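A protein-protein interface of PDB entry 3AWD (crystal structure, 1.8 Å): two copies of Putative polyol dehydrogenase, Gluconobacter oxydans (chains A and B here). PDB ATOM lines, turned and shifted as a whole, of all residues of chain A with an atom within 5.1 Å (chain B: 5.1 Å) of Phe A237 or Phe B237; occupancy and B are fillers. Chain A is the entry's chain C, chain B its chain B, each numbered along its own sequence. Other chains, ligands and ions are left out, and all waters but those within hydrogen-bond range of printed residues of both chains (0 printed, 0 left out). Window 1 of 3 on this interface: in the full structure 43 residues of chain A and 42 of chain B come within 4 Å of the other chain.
O of Phe B237 lies within hydrogen-bond range of OG of Ser B240.
The backbone NH of Ala B242 sits close to the side-chain hydroxyl of Ser B240, 3.2 Å away.
The side-chain hydroxyl (OG) of Ser A240 lies within hydrogen-bond range of the backbone carbonyl oxygen (O) of Phe A237, at 2.7 Å.
The side-chain hydroxyl (OG) of Ser A240 lies close to the backbone NH (N) of Ala A242 (3.2 Å).
Printed residues of chain B within 4 Å of Ser A233: Phe B237 and Ala B242.
Phe A237 touches just these residues of chain B: Ser B233, Val B234 and Phe B237.
Of the printed residues of chain B, Ala A242 touches Ser B233.
Of chain A, only Ser A233, Val A234 and Phe A237 come within 4 Å of Phe B237.
Of the printed residues of chain A, Met B246 touches Val A234.
The nearest printed residue of chain B that does not touch Val A234 is Ala B242 (4.4 Å).
Ser A233 touches Ala B242, and with the chains exchanged Ala A242 touches Ser B233.
Val A234 touches Phe B237, and with the chains exchanged Phe A237 touches Val B234.
Val A234 touches Met B246, and with the chains exchanged Met A246 touches Val B234.
Phe B237 touches its own counterpart, Phe A237.
Of the 9 pairs that touch across the chains among the printed residues, 9 have their exchanged pair printed and touching as well.
Of the 13 printed residues of chain B, 5 touch a printed residue of chain A.
Along chain B the printed residues that touch a printed residue of chain A span positions 233 to 246.
Of the 13 printed residues of chain A, 5 touch a printed residue of chain B.
Printed residues of chain A that touch a printed residue of chain B: Ser A233, Val A234, Phe A237, Ala A242 and Met A246.
Among the printed residues, 9 pairs touch across the chains.
Among the printed residues, no Asp or Glu carboxylate lies within 4 Å of a Lys or Arg side-chain nitrogen of the other chain.
Among the printed residues, merely in contact across the chains: Ser A233 with Ala B242 (3.2 Å), Ala A242 with Ser B233 (3.3 Å), Phe A237 with Phe B237 (3.6 Å), Ser A233 with Phe B237 (3.7 Å), Phe A237 with Val B234 (3.7 Å), Phe A237 with Ser B233 (3.8 Å), Val A234 with Phe B237 (3.8 Å), Met A246 with Val B234 (3.9 Å) and Val A234 with Met B246 (3.9 Å).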
ATOM      1  N   LEU A   9      14.946  17.403  29.464  1.00  0.00           N
ATOM      2  CA  LEU A   9      14.876  16.939  28.080  1.00  0.00           C
ATOM      3  C   LEU A   9      15.627  15.602  27.829  1.00  0.00           C
ATOM      4  O   LEU A   9      15.392  14.918  26.817  1.00  0.00           O
ATOM      5  CB  LEU A   9      15.346  18.063  27.139  1.00  0.00           C
ATOM      6  CG  LEU A   9      14.418  19.307  27.182  1.00  0.00           C
ATOM      7  CD1 LEU A   9      15.115  20.627  26.829  1.00  0.00           C
ATOM      8  CD2 LEU A   9      13.199  19.094  26.292  1.00  0.00           C
ATOM      9  N   ALA A 232       9.881  14.560  14.704  1.00  0.00           N
ATOM     10  CA  ALA A 232      10.703  13.852  15.696  1.00  0.00           C
ATOM     11  C   ALA A 232      11.024  14.740  16.895  1.00  0.00           C
ATOM     12  O   ALA A 232      11.040  14.268  18.050  1.00  0.00           O
ATOM     13  CB  ALA A 232      11.978  13.334  15.047  1.00  0.00           C
ATOM     14  N   SER A 233      11.294  16.026  16.635  1.00  0.00           N
ATOM     15  CA  SER A 233      11.582  16.957  17.742  1.00  0.00           C
ATOM     16  C   SER A 233      10.422  17.040  18.745  1.00  0.00           C
ATOM     17  O   SER A 233      10.642  17.048  19.971  1.00  0.00           O
ATOM     18  CB  SER A 233      11.928  18.348  17.208  1.00  0.00           C
ATOM     19  OG  SER A 233      13.289  18.408  16.813  1.00  0.00           O
ATOM     20  N   VAL A 234       9.194  17.089  18.226  1.00  0.00           N
ATOM     21  CA  VAL A 234       8.018  17.176  19.110  1.00  0.00           C
ATOM     22  C   VAL A 234       7.805  15.854  19.853  1.00  0.00           C
ATOM     23  O   VAL A 234       7.476  15.850  21.043  1.00  0.00           O
ATOM     24  CB  VAL A 234       6.741  17.616  18.345  1.00  0.00           C
ATOM     25  CG1 VAL A 234       5.542  17.805  19.323  1.00  0.00           C
ATOM     26  CG2 VAL A 234       7.005  18.928  17.564  1.00  0.00           C
ATOM     27  N   VAL A 235       7.974  14.750  19.131  1.00  0.00           N
ATOM     28  CA  VAL A 235       7.844  13.412  19.715  1.00  0.00           C
ATOM     29  C   VAL A 235       8.824  13.226  20.889  1.00  0.00           C
ATOM     30  O   VAL A 235       8.432  12.759  21.961  1.00  0.00           O
ATOM     31  CB  VAL A 235       8.016  12.327  18.637  1.00  0.00           C
ATOM     32  CG1 VAL A 235       8.150  10.904  19.288  1.00  0.00           C
ATOM     33  CG2 VAL A 235       6.820  12.366  17.668  1.00  0.00           C
ATOM     34  N   GLN A 236      10.085  13.616  20.679  1.00  0.00           N
ATOM     35  CA  GLN A 236      11.124  13.494  21.707  1.00  0.00           C
ATOM     36  C   GLN A 236      10.730  14.349  22.903  1.00  0.00           C
ATOM     37  O   GLN A 236      10.834  13.914  24.049  1.00  0.00           O
ATOM     38  CB  GLN A 236      12.498  13.906  21.133  1.00  0.00           C
ATOM     39  CG  GLN A 236      13.715  13.641  22.101  1.00  0.00           C
ATOM     40  CD  GLN A 236      13.844  14.694  23.191  1.00  0.00           C
ATOM     41  OE1 GLN A 236      13.605  15.880  22.949  1.00  0.00           O
ATOM     42  NE2 GLN A 236      14.204  14.261  24.411  1.00  0.00           N
ATOM     43  N   PHE A 237      10.238  15.560  22.641  1.00  0.00           N
ATOM     44  CA  PHE A 237       9.823  16.426  23.732  1.00  0.00           C
ATOM     45  C   PHE A 237       8.724  15.759  24.566  1.00  0.00           C
ATOM     46  O   PHE A 237       8.798  15.700  25.814  1.00  0.00           O
ATOM     47  CB  PHE A 237       9.326  17.773  23.216  1.00  0.00           C
ATOM     48  CG  PHE A 237       8.795  18.652  24.309  1.00  0.00           C
ATOM     49  CD1 PHE A 237       9.672  19.321  25.155  1.00  0.00           C
ATOM     50  CD2 PHE A 237       7.416  18.762  24.530  1.00  0.00           C
ATOM     51  CE1 PHE A 237       9.194  20.127  26.195  1.00  0.00           C
ATOM     52  CE2 PHE A 237       6.930  19.554  25.571  1.00  0.00           C
ATOM     53  CZ  PHE A 237       7.822  20.229  26.401  1.00  0.00           C
ATOM     54  N   LEU A 238       7.704  15.268  23.868  1.00  0.00           N
ATOM     55  CA  LEU A 238       6.557  14.601  24.516  1.00  0.00           C
ATOM     56  C   LEU A 238       6.918  13.342  25.289  1.00  0.00           C
ATOM     57  O   LEU A 238       6.233  12.978  26.239  1.00  0.00           O
ATOM     58  CB  LEU A 238       5.480  14.267  23.471  1.00  0.00           C
ATOM     59  CG  LEU A 238       4.747  15.492  22.894  1.00  0.00           C
ATOM     60  CD1 LEU A 238       3.829  15.053  21.763  1.00  0.00           C
ATOM     61  CD2 LEU A 238       3.960  16.228  24.012  1.00  0.00           C
ATOM     62  N   ALA A 239       7.991  12.690  24.871  1.00  0.00           N
ATOM     63  CA  ALA A 239       8.496  11.487  25.549  1.00  0.00           C
ATOM     64  C   ALA A 239       9.293  11.806  26.824  1.00  0.00           C
ATOM     65  O   ALA A 239       9.562  10.918  27.628  1.00  0.00           O
ATOM     66  CB  ALA A 239       9.343  10.691  24.573  1.00  0.00           C
ATOM     67  N   SER A 240       9.662  13.071  26.994  1.00  0.00           N
ATOM     68  CA  SER A 240      10.585  13.495  28.048  1.00  0.00           C
ATOM     69  C   SER A 240       9.834  14.057  29.241  1.00  0.00           C
ATOM     70  O   SER A 240       8.665  14.427  29.130  1.00  0.00           O
ATOM     71  CB  SER A 240      11.554  14.556  27.501  1.00  0.00           C
ATOM     72  OG  SER A 240      10.963  15.866  27.492  1.00  0.00           O
ATOM     73  N   ALA A 242      10.180  16.890  30.405  1.00  0.00           N
ATOM     74  CA  ALA A 242       9.799  18.282  30.150  1.00  0.00           C
ATOM     75  C   ALA A 242       8.291  18.361  29.888  1.00  0.00           C
ATOM     76  O   ALA A 242       7.665  19.372  30.184  1.00  0.00           O
ATOM     77  CB  ALA A 242      10.591  18.877  28.950  1.00  0.00           C
ATOM     78  N   ALA A 243       7.719  17.279  29.358  1.00  0.00           N
ATOM     79  CA  ALA A 243       6.281  17.203  29.086  1.00  0.00           C
ATOM     80  C   ALA A 243       5.475  16.550  30.225  1.00  0.00           C
ATOM     81  O   ALA A 243       4.384  15.994  29.985  1.00  0.00           O
ATOM     82  CB  ALA A 243       6.030  16.489  27.766  1.00  0.00           C
ATOM     83  N   MET A 246       1.724  17.079  30.465  1.00  0.00           N
ATOM     84  CA  MET A 246       0.942  16.822  29.252  1.00  0.00           C
ATOM     85  C   MET A 246       0.499  15.372  29.152  1.00  0.00           C
ATOM     86  O   MET A 246       1.328  14.481  29.089  1.00  0.00           O
ATOM     87  CB  MET A 246       1.740  17.193  28.009  1.00  0.00           C
ATOM     88  CG  MET A 246       1.965  18.714  27.864  1.00  0.00           C
ATOM     89  SD  MET A 246       2.878  19.080  26.374  1.00  0.00           S
ATOM     90  CE  MET A 246       1.611  18.743  25.134  1.00  0.00           C
ATOM     91  N   LEU B   9      17.069  22.912  20.709  1.00  0.00           N
ATOM     92  CA  LEU B   9      16.409  23.395  21.917  1.00  0.00           C
ATOM     93  C   LEU B   9      17.073  24.660  22.494  1.00  0.00           C
ATOM     94  O   LEU B   9      16.508  25.307  23.371  1.00  0.00           O
ATOM     95  CB  LEU B   9      16.316  22.252  22.953  1.00  0.00           C
ATOM     96  CG  LEU B   9      15.449  21.090  22.383  1.00  0.00           C
ATOM     97  CD1 LEU B   9      15.854  19.731  22.923  1.00  0.00           C
ATOM     98  CD2 LEU B   9      13.981  21.359  22.677  1.00  0.00           C
ATOM     99  N   ALA B 232       6.449  26.212  31.945  1.00  0.00           N
ATOM    100  CA  ALA B 232       7.640  26.856  31.400  1.00  0.00           C
ATOM    101  C   ALA B 232       8.389  25.932  30.459  1.00  0.00           C
ATOM    102  O   ALA B 232       8.922  26.383  29.460  1.00  0.00           O
ATOM    103  CB  ALA B 232       8.550  27.318  32.527  1.00  0.00           C
ATOM    104  N   SER B 233       8.438  24.637  30.776  1.00  0.00           N
ATOM    105  CA  SER B 233       9.099  23.681  29.883  1.00  0.00           C
ATOM    106  C   SER B 233       8.466  23.671  28.486  1.00  0.00           C
ATOM    107  O   SER B 233       9.177  23.670  27.471  1.00  0.00           O
ATOM    108  CB  SER B 233       9.072  22.288  30.501  1.00  0.00           C
ATOM    109  OG  SER B 233      10.109  22.160  31.476  1.00  0.00           O
ATOM    110  N   VAL B 234       7.132  23.666  28.439  1.00  0.00           N
ATOM    111  CA  VAL B 234       6.420  23.623  27.145  1.00  0.00           C
ATOM    112  C   VAL B 234       6.625  24.956  26.447  1.00  0.00           C
ATOM    113  O   VAL B 234       6.807  25.013  25.216  1.00  0.00           O
ATOM    114  CB  VAL B 234       4.915  23.307  27.319  1.00  0.00           C
ATOM    115  CG1 VAL B 234       4.204  23.193  25.933  1.00  0.00           C
ATOM    116  CG2 VAL B 234       4.722  21.998  28.132  1.00  0.00           C
ATOM    117  N   VAL B 235       6.588  26.043  27.218  1.00  0.00           N
ATOM    118  CA  VAL B 235       6.766  27.371  26.603  1.00  0.00           C
ATOM    119  C   VAL B 235       8.161  27.490  25.961  1.00  0.00           C
ATOM    120  O   VAL B 235       8.298  27.957  24.823  1.00  0.00           O
ATOM    121  CB  VAL B 235       6.522  28.512  27.623  1.00  0.00           C
ATOM    122  CG1 VAL B 235       6.986  29.877  27.072  1.00  0.00           C
ATOM    123  CG2 VAL B 235       5.048  28.583  28.003  1.00  0.00           C
ATOM    124  N   GLN B 236       9.180  27.053  26.687  1.00  0.00           N
ATOM    125  CA  GLN B 236      10.562  27.100  26.195  1.00  0.00           C
ATOM    126  C   GLN B 236      10.696  26.285  24.914  1.00  0.00           C
ATOM    127  O   GLN B 236      11.313  26.745  23.938  1.00  0.00           O
ATOM    128  CB  GLN B 236      11.538  26.597  27.279  1.00  0.00           C
ATOM    129  CG  GLN B 236      13.036  26.805  26.932  1.00  0.00           C
ATOM    130  CD  GLN B 236      13.573  25.736  25.968  1.00  0.00           C
ATOM    131  OE1 GLN B 236      13.197  24.571  26.048  1.00  0.00           O
ATOM    132  NE2 GLN B 236      14.468  26.146  25.057  1.00  0.00           N
ATOM    133  N   PHE B 237      10.087  25.099  24.904  1.00  0.00           N
ATOM    134  CA  PHE B 237      10.095  24.274  23.695  1.00  0.00           C
ATOM    135  C   PHE B 237       9.480  25.008  22.489  1.00  0.00           C
ATOM    136  O   PHE B 237      10.063  25.067  21.408  1.00  0.00           O
ATOM    137  CB  PHE B 237       9.377  22.934  23.927  1.00  0.00           C
ATOM    138  CG  PHE B 237       9.291  22.087  22.671  1.00  0.00           C
ATOM    139  CD1 PHE B 237      10.387  21.350  22.246  1.00  0.00           C
ATOM    140  CD2 PHE B 237       8.129  22.076  21.904  1.00  0.00           C
ATOM    141  CE1 PHE B 237      10.327  20.575  21.087  1.00  0.00           C
ATOM    142  CE2 PHE B 237       8.048  21.314  20.721  1.00  0.00           C
ATOM    143  CZ  PHE B 237       9.163  20.571  20.318  1.00  0.00           C
ATOM    144  N   LEU B 238       8.302  25.589  22.695  1.00  0.00           N
ATOM    145  CA  LEU B 238       7.586  26.290  21.630  1.00  0.00           C
ATOM    146  C   LEU B 238       8.326  27.524  21.127  1.00  0.00           C
ATOM    147  O   LEU B 238       8.151  27.938  19.973  1.00  0.00           O
ATOM    148  CB  LEU B 238       6.185  26.673  22.111  1.00  0.00           C
ATOM    149  CG  LEU B 238       5.245  25.478  22.331  1.00  0.00           C
ATOM    150  CD1 LEU B 238       3.950  25.960  22.999  1.00  0.00           C
ATOM    151  CD2 LEU B 238       4.929  24.818  20.957  1.00  0.00           C
ATOM    152  N   ALA B 239       9.168  28.094  21.972  1.00  0.00           N
ATOM    153  CA  ALA B 239       9.970  29.266  21.582  1.00  0.00           C
ATOM    154  C   ALA B 239      11.198  28.846  20.768  1.00  0.00           C
ATOM    155  O   ALA B 239      11.835  29.679  20.130  1.00  0.00           O
ATOM    156  CB  ALA B 239      10.395  30.045  22.856  1.00  0.00           C
ATOM    157  N   SER B 240      11.542  27.556  20.801  1.00  0.00           N
ATOM    158  CA  SER B 240      12.798  27.076  20.212  1.00  0.00           C
ATOM    159  C   SER B 240      12.594  26.576  18.781  1.00  0.00           C
ATOM    160  O   SER B 240      11.450  26.310  18.362  1.00  0.00           O
ATOM    161  CB  SER B 240      13.400  25.952  21.060  1.00  0.00           C
ATOM    162  OG  SER B 240      12.732  24.721  20.783  1.00  0.00           O
ATOM    163  N   ALA B 242      13.217  23.714  17.779  1.00  0.00           N
ATOM    164  CA  ALA B 242      12.664  22.363  17.836  1.00  0.00           C
ATOM    165  C   ALA B 242      11.177  22.338  17.431  1.00  0.00           C
ATOM    166  O   ALA B 242      10.686  21.332  16.907  1.00  0.00           O
ATOM    167  CB  ALA B 242      12.852  21.753  19.239  1.00  0.00           C
ATOM    168  N   ALA B 243      10.472  23.437  17.704  1.00  0.00           N
ATOM    169  CA  ALA B 243       9.048  23.595  17.364  1.00  0.00           C
ATOM    170  C   ALA B 243       8.837  24.278  15.988  1.00  0.00           C
ATOM    171  O   ALA B 243       7.805  24.909  15.737  1.00  0.00           O
ATOM    172  CB  ALA B 243       8.344  24.387  18.481  1.00  0.00           C
ATOM    173  N   MET B 246       5.550  23.992  14.206  1.00  0.00           N
ATOM    174  CA  MET B 246       4.347  24.329  14.950  1.00  0.00           C
ATOM    175  C   MET B 246       4.001  25.825  14.870  1.00  0.00           C
ATOM    176  O   MET B 246       4.786  26.680  15.310  1.00  0.00           O
ATOM    177  CB  MET B 246       4.481  23.917  16.425  1.00  0.00           C
ATOM    178  CG  MET B 246       4.681  22.415  16.670  1.00  0.00           C
ATOM    179  SD  MET B 246       4.755  21.969  18.416  1.00  0.00           S
ATOM    180  CE  MET B 246       3.087  22.363  18.966  1.00  0.00           C
